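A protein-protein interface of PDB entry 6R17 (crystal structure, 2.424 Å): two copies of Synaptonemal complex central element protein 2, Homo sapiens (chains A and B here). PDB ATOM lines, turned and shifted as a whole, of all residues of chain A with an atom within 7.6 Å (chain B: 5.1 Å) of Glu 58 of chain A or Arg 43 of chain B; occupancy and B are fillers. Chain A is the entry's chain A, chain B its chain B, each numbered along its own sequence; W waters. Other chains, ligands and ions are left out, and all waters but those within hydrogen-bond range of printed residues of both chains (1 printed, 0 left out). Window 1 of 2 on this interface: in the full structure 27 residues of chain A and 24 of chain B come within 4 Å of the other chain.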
ATOM      1  N   LYS A  47      -4.491  24.537 -18.038  1.00  0.00           N
ATOM      2  CA  LYS A  47      -4.240  25.077 -16.705  1.00  0.00           C
ATOM      3  C   LYS A  47      -4.944  24.247 -15.636  1.00  0.00           C
ATOM      4  O   LYS A  47      -4.398  24.033 -14.547  1.00  0.00           O
ATOM      5  CB  LYS A  47      -4.665  26.544 -16.642  1.00  0.00           C
ATOM      6  CG  LYS A  47      -3.677  27.473 -17.336  1.00  0.00           C
ATOM      7  CD  LYS A  47      -4.073  28.934 -17.218  1.00  0.00           C
ATOM      8  CE  LYS A  47      -2.919  29.835 -17.629  1.00  0.00           C
ATOM      9  NZ  LYS A  47      -2.330  29.423 -18.933  1.00  0.00           N
ATOM     10  N   THR A  48      -6.156  23.770 -15.927  1.00  0.00           N
ATOM     11  CA  THR A  48      -6.861  22.912 -14.976  1.00  0.00           C
ATOM     12  C   THR A  48      -6.099  21.608 -14.748  1.00  0.00           C
ATOM     13  O   THR A  48      -5.984  21.130 -13.610  1.00  0.00           O
ATOM     14  CB  THR A  48      -8.281  22.633 -15.475  1.00  0.00           C
ATOM     15  OG1 THR A  48      -9.113  23.773 -15.219  1.00  0.00           O
ATOM     16  CG2 THR A  48      -8.875  21.410 -14.787  1.00  0.00           C
ATOM     17  N   VAL A  50      -2.875  21.181 -15.081  1.00  0.00           N
ATOM     18  CA  VAL A  50      -1.693  21.532 -14.293  1.00  0.00           C
ATOM     19  C   VAL A  50      -2.065  21.689 -12.824  1.00  0.00           C
ATOM     20  O   VAL A  50      -1.307  21.298 -11.927  1.00  0.00           O
ATOM     21  CB  VAL A  50      -1.038  22.810 -14.853  1.00  0.00           C
ATOM     22  CG1 VAL A  50       0.109  23.260 -13.959  1.00  0.00           C
ATOM     23  CG2 VAL A  50      -0.543  22.577 -16.270  1.00  0.00           C
ATOM     24  N   SER A  51      -3.233  22.278 -12.556  1.00  0.00           N
ATOM     25  CA  SER A  51      -3.711  22.382 -11.181  1.00  0.00           C
ATOM     26  C   SER A  51      -3.912  21.004 -10.568  1.00  0.00           C
ATOM     27  O   SER A  51      -3.578  20.782  -9.400  1.00  0.00           O
ATOM     28  CB  SER A  51      -5.010  23.187 -11.134  1.00  0.00           C
ATOM     29  OG  SER A  51      -5.450  23.361  -9.798  1.00  0.00           O
ATOM     30  N   ASP A  52      -4.454  20.061 -11.344  1.00  0.00           N
ATOM     31  CA  ASP A  52      -4.623  18.698 -10.842  1.00  0.00           C
ATOM     32  C   ASP A  52      -3.276  18.059 -10.517  1.00  0.00           C
ATOM     33  O   ASP A  52      -3.133  17.358  -9.504  1.00  0.00           O
ATOM     34  CB  ASP A  52      -5.381  17.847 -11.861  1.00  0.00           C
ATOM     35  CG  ASP A  52      -6.797  18.330 -12.088  1.00  0.00           C
ATOM     36  OD1 ASP A  52      -7.281  19.153 -11.283  1.00  0.00           O
ATOM     37  OD2 ASP A  52      -7.427  17.885 -13.071  1.00  0.00           O
ATOM     38  N   LEU A  53      -2.275  18.287 -11.370  1.00  0.00           N
ATOM     39  CA  LEU A  53      -0.957  17.707 -11.119  1.00  0.00           C
ATOM     40  C   LEU A  53      -0.321  18.300  -9.865  1.00  0.00           C
ATOM     41  O   LEU A  53       0.255  17.571  -9.045  1.00  0.00           O
ATOM     42  CB  LEU A  53      -0.049  17.918 -12.330  1.00  0.00           C
ATOM     43  CG  LEU A  53      -0.526  17.323 -13.655  1.00  0.00           C
ATOM     44  CD1 LEU A  53       0.408  17.711 -14.790  1.00  0.00           C
ATOM     45  CD2 LEU A  53      -0.654  15.812 -13.552  1.00  0.00           C
ATOM     46  N   THR A  54      -0.419  19.623  -9.704  1.00  0.00           N
ATOM     47  CA  THR A  54       0.061  20.261  -8.481  1.00  0.00           C
ATOM     48  C   THR A  54      -0.674  19.714  -7.263  1.00  0.00           C
ATOM     49  O   THR A  54      -0.074  19.513  -6.199  1.00  0.00           O
ATOM     50  CB  THR A  54      -0.123  21.775  -8.575  1.00  0.00           C
ATOM     51  OG1 THR A  54       0.525  22.265  -9.754  1.00  0.00           O
ATOM     52  CG2 THR A  54       0.500  22.458  -7.366  1.00  0.00           C
ATOM     53  N   GLU A  55      -1.976  19.461  -7.411  1.00  0.00           N
ATOM     54  CA  GLU A  55      -2.779  18.913  -6.325  1.00  0.00           C
ATOM     55  C   GLU A  55      -2.257  17.548  -5.892  1.00  0.00           C
ATOM     56  O   GLU A  55      -2.093  17.282  -4.695  1.00  0.00           O
ATOM     57  CB  GLU A  55      -4.237  18.824  -6.780  1.00  0.00           C
ATOM     58  CG  GLU A  55      -5.229  18.359  -5.735  1.00  0.00           C
ATOM     59  CD  GLU A  55      -6.620  18.178  -6.318  1.00  0.00           C
ATOM     60  OE1 GLU A  55      -6.924  18.828  -7.341  1.00  0.00           O
ATOM     61  OE2 GLU A  55      -7.407  17.386  -5.758  1.00  0.00           O
ATOM     62  N   LYS A  56      -1.982  16.668  -6.858  1.00  0.00           N
ATOM     63  CA  LYS A  56      -1.477  15.338  -6.514  1.00  0.00           C
ATOM     64  C   LYS A  56      -0.077  15.407  -5.911  1.00  0.00           C
ATOM     65  O   LYS A  56       0.252  14.633  -4.998  1.00  0.00           O
ATOM     66  CB  LYS A  56      -1.510  14.422  -7.737  1.00  0.00           C
ATOM     67  CG  LYS A  56      -2.879  14.371  -8.392  1.00  0.00           C
ATOM     68  CD  LYS A  56      -3.901  13.804  -7.418  1.00  0.00           C
ATOM     69  CE  LYS A  56      -5.299  14.330  -7.698  1.00  0.00           C
ATOM     70  NZ  LYS A  56      -6.212  14.115  -6.538  1.00  0.00           N
ATOM     71  N   LEU A  57       0.765  16.318  -6.409  1.00  0.00           N
ATOM     72  CA  LEU A  57       2.082  16.499  -5.802  1.00  0.00           C
ATOM     73  C   LEU A  57       1.955  16.911  -4.340  1.00  0.00           C
ATOM     74  O   LEU A  57       2.639  16.362  -3.463  1.00  0.00           O
ATOM     75  CB  LEU A  57       2.892  17.535  -6.581  1.00  0.00           C
ATOM     76  CG  LEU A  57       3.716  17.021  -7.761  1.00  0.00           C
ATOM     77  CD1 LEU A  57       4.552  18.146  -8.350  1.00  0.00           C
ATOM     78  CD2 LEU A  57       4.603  15.865  -7.319  1.00  0.00           C
ATOM     79  N   GLU A  58       1.082  17.883  -4.061  1.00  0.00           N
ATOM     80  CA  GLU A  58       0.875  18.305  -2.681  1.00  0.00           C
ATOM     81  C   GLU A  58       0.319  17.169  -1.835  1.00  0.00           C
ATOM     82  O   GLU A  58       0.678  17.029  -0.663  1.00  0.00           O
ATOM     83  CB  GLU A  58      -0.060  19.514  -2.627  1.00  0.00           C
ATOM     84  CG  GLU A  58       0.467  20.744  -3.340  1.00  0.00           C
ATOM     85  CD  GLU A  58      -0.561  21.853  -3.424  1.00  0.00           C
ATOM     86  OE1 GLU A  58      -0.167  23.007  -3.690  1.00  0.00           O
ATOM     87  OE2 GLU A  58      -1.761  21.575  -3.212  1.00  0.00           O
ATOM     88  N   GLU A  59      -0.541  16.331  -2.421  1.00  0.00           N
ATOM     89  CA  GLU A  59      -1.085  15.194  -1.684  1.00  0.00           C
ATOM     90  C   GLU A  59       0.017  14.225  -1.260  1.00  0.00           C
ATOM     91  O   GLU A  59       0.092  13.818  -0.092  1.00  0.00           O
ATOM     92  CB  GLU A  59      -2.141  14.490  -2.539  1.00  0.00           C
ATOM     93  CG  GLU A  59      -2.507  13.087  -2.090  1.00  0.00           C
ATOM     94  CD  GLU A  59      -3.502  12.427  -3.028  1.00  0.00           C
ATOM     95  OE1 GLU A  59      -3.945  13.094  -3.989  1.00  0.00           O
ATOM     96  OE2 GLU A  59      -3.844  11.247  -2.804  1.00  0.00           O
ATOM     97  N   ARG A  60       0.892  13.849  -2.198  1.00  0.00           N
ATOM     98  CA  ARG A  60       1.965  12.915  -1.851  1.00  0.00           C
ATOM     99  C   ARG A  60       2.951  13.518  -0.854  1.00  0.00           C
ATOM    100  O   ARG A  60       3.388  12.839   0.088  1.00  0.00           O
ATOM    101  CB  ARG A  60       2.704  12.448  -3.103  1.00  0.00           C
ATOM    102  CG  ARG A  60       3.544  11.211  -2.838  1.00  0.00           C
ATOM    103  CD  ARG A  60       3.970  10.499  -4.106  1.00  0.00           C
ATOM    104  NE  ARG A  60       2.924   9.617  -4.619  1.00  0.00           N
ATOM    105  CZ  ARG A  60       2.555   8.474  -4.045  1.00  0.00           C
ATOM    106  NH1 ARG A  60       3.134   8.068  -2.921  1.00  0.00           N
ATOM    107  NH2 ARG A  60       1.597   7.738  -4.590  1.00  0.00           N
ATOM    108  N   ILE A  61       3.316  14.790  -1.041  1.00  0.00           N
ATOM    109  CA  ILE A  61       4.227  15.431  -0.097  1.00  0.00           C
ATOM    110  C   ILE A  61       3.593  15.500   1.284  1.00  0.00           C
ATOM    111  O   ILE A  61       4.267  15.315   2.308  1.00  0.00           O
ATOM    112  CB  ILE A  61       4.638  16.818  -0.616  1.00  0.00           C
ATOM    113  CG1 ILE A  61       5.433  16.658  -1.911  1.00  0.00           C
ATOM    114  CG2 ILE A  61       5.474  17.541   0.423  1.00  0.00           C
ATOM    115  CD1 ILE A  61       5.439  17.881  -2.781  1.00  0.00           C
ATOM    116  N   TYR A  62       2.287  15.768   1.337  1.00  0.00           N
ATOM    117  CA  TYR A  62       1.604  15.794   2.620  1.00  0.00           C
ATOM    118  C   TYR A  62       1.631  14.425   3.282  1.00  0.00           C
ATOM    119  O   TYR A  62       1.786  14.327   4.502  1.00  0.00           O
ATOM    120  CB  TYR A  62       0.162  16.271   2.460  1.00  0.00           C
ATOM    121  CG  TYR A  62      -0.563  16.200   3.773  1.00  0.00           C
ATOM    122  CD1 TYR A  62      -0.455  17.234   4.687  1.00  0.00           C
ATOM    123  CD2 TYR A  62      -1.325  15.089   4.119  1.00  0.00           C
ATOM    124  CE1 TYR A  62      -1.086  17.175   5.899  1.00  0.00           C
ATOM    125  CE2 TYR A  62      -1.963  15.022   5.336  1.00  0.00           C
ATOM    126  CZ  TYR A  62      -1.839  16.074   6.217  1.00  0.00           C
ATOM    127  OH  TYR A  62      -2.458  16.037   7.432  1.00  0.00           O
ATOM    128  N   GLN A  63       1.448  13.358   2.501  1.00  0.00           N
ATOM    129  CA  GLN A  63       1.524  12.019   3.083  1.00  0.00           C
ATOM    130  C   GLN A  63       2.913  11.747   3.655  1.00  0.00           C
ATOM    131  O   GLN A  63       3.047  11.155   4.735  1.00  0.00           O
ATOM    132  CB  GLN A  63       1.144  10.964   2.045  1.00  0.00           C
ATOM    133  CG  GLN A  63      -0.353  10.857   1.784  1.00  0.00           C
ATOM    134  CD  GLN A  63      -1.143  10.518   3.037  1.00  0.00           C
ATOM    135  OE1 GLN A  63      -1.546  11.404   3.792  1.00  0.00           O
ATOM    136  NE2 GLN A  63      -1.371   9.228   3.261  1.00  0.00           N
ATOM    137  N   ILE A  64       3.957  12.188   2.949  1.00  0.00           N
ATOM    138  CA  ILE A  64       5.320  12.015   3.455  1.00  0.00           C
ATOM    139  C   ILE A  64       5.502  12.760   4.775  1.00  0.00           C
ATOM    140  O   ILE A  64       6.051  12.220   5.746  1.00  0.00           O
ATOM    141  CB  ILE A  64       6.348  12.469   2.403  1.00  0.00           C
ATOM    142  CG1 ILE A  64       6.216  11.629   1.133  1.00  0.00           C
ATOM    143  CG2 ILE A  64       7.761  12.385   2.966  1.00  0.00           C
ATOM    144  CD1 ILE A  64       7.182  12.024   0.041  1.00  0.00           C
ATOM    145  N   MET B  39       6.189  25.871   0.568  1.00  0.00           N
ATOM    146  CA  MET B  39       5.357  25.101  -0.362  1.00  0.00           C
ATOM    147  C   MET B  39       4.392  26.001  -1.131  1.00  0.00           C
ATOM    148  O   MET B  39       4.228  25.865  -2.355  1.00  0.00           O
ATOM    149  CB  MET B  39       4.580  24.020   0.388  1.00  0.00           C
ATOM    150  CG  MET B  39       3.437  23.427  -0.429  1.00  0.00           C
ATOM    151  SD  MET B  39       2.641  21.996   0.327  1.00  0.00           S
ATOM    152  CE  MET B  39       3.964  20.792   0.247  1.00  0.00           C
ATOM    153  N   THR B  40       3.718  26.902  -0.416  1.00  0.00           N
ATOM    154  CA  THR B  40       2.847  27.879  -1.059  1.00  0.00           C
ATOM    155  C   THR B  40       3.626  28.720  -2.059  1.00  0.00           C
ATOM    156  O   THR B  40       3.110  29.056  -3.137  1.00  0.00           O
ATOM    157  CB  THR B  40       2.178  28.752  -0.001  1.00  0.00           C
ATOM    158  OG1 THR B  40       3.184  29.349   0.827  1.00  0.00           O
ATOM    159  CG2 THR B  40       1.263  27.891   0.875  1.00  0.00           C
ATOM    160  N   ASN B  41       4.869  29.090  -1.716  1.00  0.00           N
ATOM    161  CA  ASN B  41       5.667  29.846  -2.682  1.00  0.00           C
ATOM    162  C   ASN B  41       5.863  29.050  -3.972  1.00  0.00           C
ATOM    163  O   ASN B  41       5.779  29.605  -5.083  1.00  0.00           O
ATOM    164  CB  ASN B  41       7.020  30.227  -2.076  1.00  0.00           C
ATOM    165  CG  ASN B  41       6.930  31.432  -1.161  1.00  0.00           C
ATOM    166  OD1 ASN B  41       5.839  31.862  -0.788  1.00  0.00           O
ATOM    167  ND2 ASN B  41       8.082  31.990  -0.799  1.00  0.00           N
ATOM    168  N   PHE B  42       6.099  27.738  -3.848  1.00  0.00           N
ATOM    169  CA  PHE B  42       6.234  26.920  -5.054  1.00  0.00           C
ATOM    170  C   PHE B  42       4.945  26.898  -5.867  1.00  0.00           C
ATOM    171  O   PHE B  42       4.986  26.964  -7.103  1.00  0.00           O
ATOM    172  CB  PHE B  42       6.638  25.482  -4.729  1.00  0.00           C
ATOM    173  CG  PHE B  42       6.555  24.559  -5.926  1.00  0.00           C
ATOM    174  CD1 PHE B  42       5.463  23.719  -6.106  1.00  0.00           C
ATOM    175  CD2 PHE B  42       7.551  24.563  -6.891  1.00  0.00           C
ATOM    176  CE1 PHE B  42       5.381  22.888  -7.212  1.00  0.00           C
ATOM    177  CE2 PHE B  42       7.474  23.733  -7.998  1.00  0.00           C
ATOM    178  CZ  PHE B  42       6.388  22.896  -8.158  1.00  0.00           C
ATOM    179  N   ARG B  43       3.793  26.738  -5.203  1.00  0.00           N
ATOM    180  CA  ARG B  43       2.556  26.684  -5.985  1.00  0.00           C
ATOM    181  C   ARG B  43       2.284  28.014  -6.678  1.00  0.00           C
ATOM    182  O   ARG B  43       1.679  28.038  -7.756  1.00  0.00           O
ATOM    183  CB  ARG B  43       1.345  26.282  -5.138  1.00  0.00           C
ATOM    184  CG  ARG B  43       0.105  26.027  -6.020  1.00  0.00           C
ATOM    185  CD  ARG B  43      -1.154  25.598  -5.274  1.00  0.00           C
ATOM    186  NE  ARG B  43      -2.308  25.568  -6.178  1.00  0.00           N
ATOM    187  CZ  ARG B  43      -2.876  24.463  -6.653  1.00  0.00           C
ATOM    188  NH1 ARG B  43      -3.914  24.552  -7.476  1.00  0.00           N
ATOM    189  NH2 ARG B  43      -2.424  23.268  -6.300  1.00  0.00           N
ATOM    190  N   ASN B  44       2.728  29.123  -6.085  1.00  0.00           N
ATOM    191  CA  ASN B  44       2.633  30.408  -6.770  1.00  0.00           C
ATOM    192  C   ASN B  44       3.462  30.400  -8.051  1.00  0.00           C
ATOM    193  O   ASN B  44       2.948  30.641  -9.163  1.00  0.00           O
ATOM    194  CB  ASN B  44       3.128  31.524  -5.844  1.00  0.00           C
ATOM    195  CG  ASN B  44       2.143  31.867  -4.750  1.00  0.00           C
ATOM    196  OD1 ASN B  44       0.986  31.450  -4.781  1.00  0.00           O
ATOM    197  ND2 ASN B  44       2.604  32.630  -3.764  1.00  0.00           N
ATOM    198  N   SER B  45       4.751  30.074  -7.908  1.00  0.00           N
ATOM    199  CA  SER B  45       5.674  30.199  -9.031  1.00  0.00           C
ATOM    200  C   SER B  45       5.368  29.219 -10.159  1.00  0.00           C
ATOM    201  O   SER B  45       5.546  29.566 -11.332  1.00  0.00           O
ATOM    202  CB  SER B  45       7.111  30.010  -8.549  1.00  0.00           C
ATOM    203  OG  SER B  45       7.276  28.750  -7.921  1.00  0.00           O
ATOM    204  N   LEU B  46       4.883  28.016  -9.842  1.00  0.00           N
ATOM    205  CA  LEU B  46       4.593  27.046 -10.897  1.00  0.00           C
ATOM    206  C   LEU B  46       3.482  27.535 -11.819  1.00  0.00           C
ATOM    207  O   LEU B  46       3.631  27.534 -13.051  1.00  0.00           O
ATOM    208  CB  LEU B  46       4.234  25.693 -10.282  1.00  0.00           C
ATOM    209  CG  LEU B  46       3.669  24.621 -11.218  1.00  0.00           C
ATOM    210  CD1 LEU B  46       4.624  24.353 -12.371  1.00  0.00           C
ATOM    211  CD2 LEU B  46       3.405  23.342 -10.444  1.00  0.00           C
ATOM    212  N   LYS B  47       2.359  27.965 -11.239  1.00  0.00           N
ATOM    213  CA  LYS B  47       1.251  28.444 -12.055  1.00  0.00           C
ATOM    214  C   LYS B  47       1.647  29.681 -12.846  1.00  0.00           C
ATOM    215  O   LYS B  47       1.350  29.783 -14.048  1.00  0.00           O
ATOM    216  CB  LYS B  47       0.042  28.752 -11.170  1.00  0.00           C
ATOM    217  CG  LYS B  47      -1.266  28.943 -11.929  1.00  0.00           C
ATOM    218  CD  LYS B  47      -2.411  29.382 -11.012  1.00  0.00           C
ATOM    219  CE  LYS B  47      -3.075  28.234 -10.245  1.00  0.00           C
ATOM    220  NZ  LYS B  47      -2.149  27.296  -9.551  1.00  0.00           N
HETATM  221  O   HOH W   1       0.042  25.515 -10.214  1.00  0.00           O
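Among the printed residues, merely in contact across the chains: Thr 54 of chain A with Leu 46 of chain B (3.2 Å), Thr 54 of chain A with Arg 43 of chain B (3.2 Å), Ile 61 of chain A with Met 39 of chain B (3.6 Å) and Glu 55 of chain A with Arg 43 of chain B (3.99 Å).
Water W1 bridges the side-chain amino group (NZ) of Lys 47 of chain B and the side-chain hydroxyl (OG1) of Thr 54 of chain A.
Of the 9 printed residues of chain B, 3 touch a printed residue of chain A.
Printed residues of chain B that touch a printed residue of chain A: Met 39, Arg 43 and Leu 46.
Hydrophobic or aromatic side chains of chain B that line the printed part of chain A: Met 39 and Leu 46.
Of the 17 printed residues of chain A, 5 touch a printed residue of chain B.
Among the printed residues, 6 pairs touch across the chains.
Among the printed residues, Asp or Glu carboxylates within 4 Å of a Lys or Arg side-chain nitrogen of the other chain: Glu 58 of chain A with Arg 43 of chain B.
The side-chain hydroxyl (OG1) of Thr 54 of chain A lies within hydrogen-bond range of the backbone carbonyl oxygen (O) of Val 50 of chain A.
OE2 of Glu 55 of chain A lies within salt-bridge range of NZ of Lys 56 of chain A (3.6 Å).
1 position is printed for both chains.
Of the 6 pairs that touch across the chains among the printed residues, none has its exchanged pair printed and touching as well.
Printed residues of chain B within 4 Å of Ser 51 of chain A: Arg 43 (3.0 Å).
Of the printed residues of chain B, Glu 55 of chain A touches Arg 43 (3.99 Å).
Glu 58 of chain A touches one residue of chain B.
Printed residues of chain B within 4 Å of Ile 61 of chain A: Met 39 (3.6 Å).
Printed residues of chain A within 4 Å of Met 39 of chain B: Ile 61.
Of the printed residues of chain A, Arg 43 of chain B touches Ser 51, Thr 54, Glu 55 and Glu 58.
The nearest residue of chain B that does not touch Glu 58 of chain A is Met 39 of chain B (4.4 Å).
The nearest printed residue of chain B that does not touch Thr 54 of chain A is Phe 42 of chain B (4.9 Å).
The guanidinium group of Arg 43 of chain B lies within hydrogen-bond range of the side-chain hydroxyl of Ser 51 of chain A (3.0 Å).
The side-chain carboxylate (OE1) of Glu 58 of chain A is in salt-bridge range of the guanidinium group (NH2) of Arg 43 of chain B (3.5 Å).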
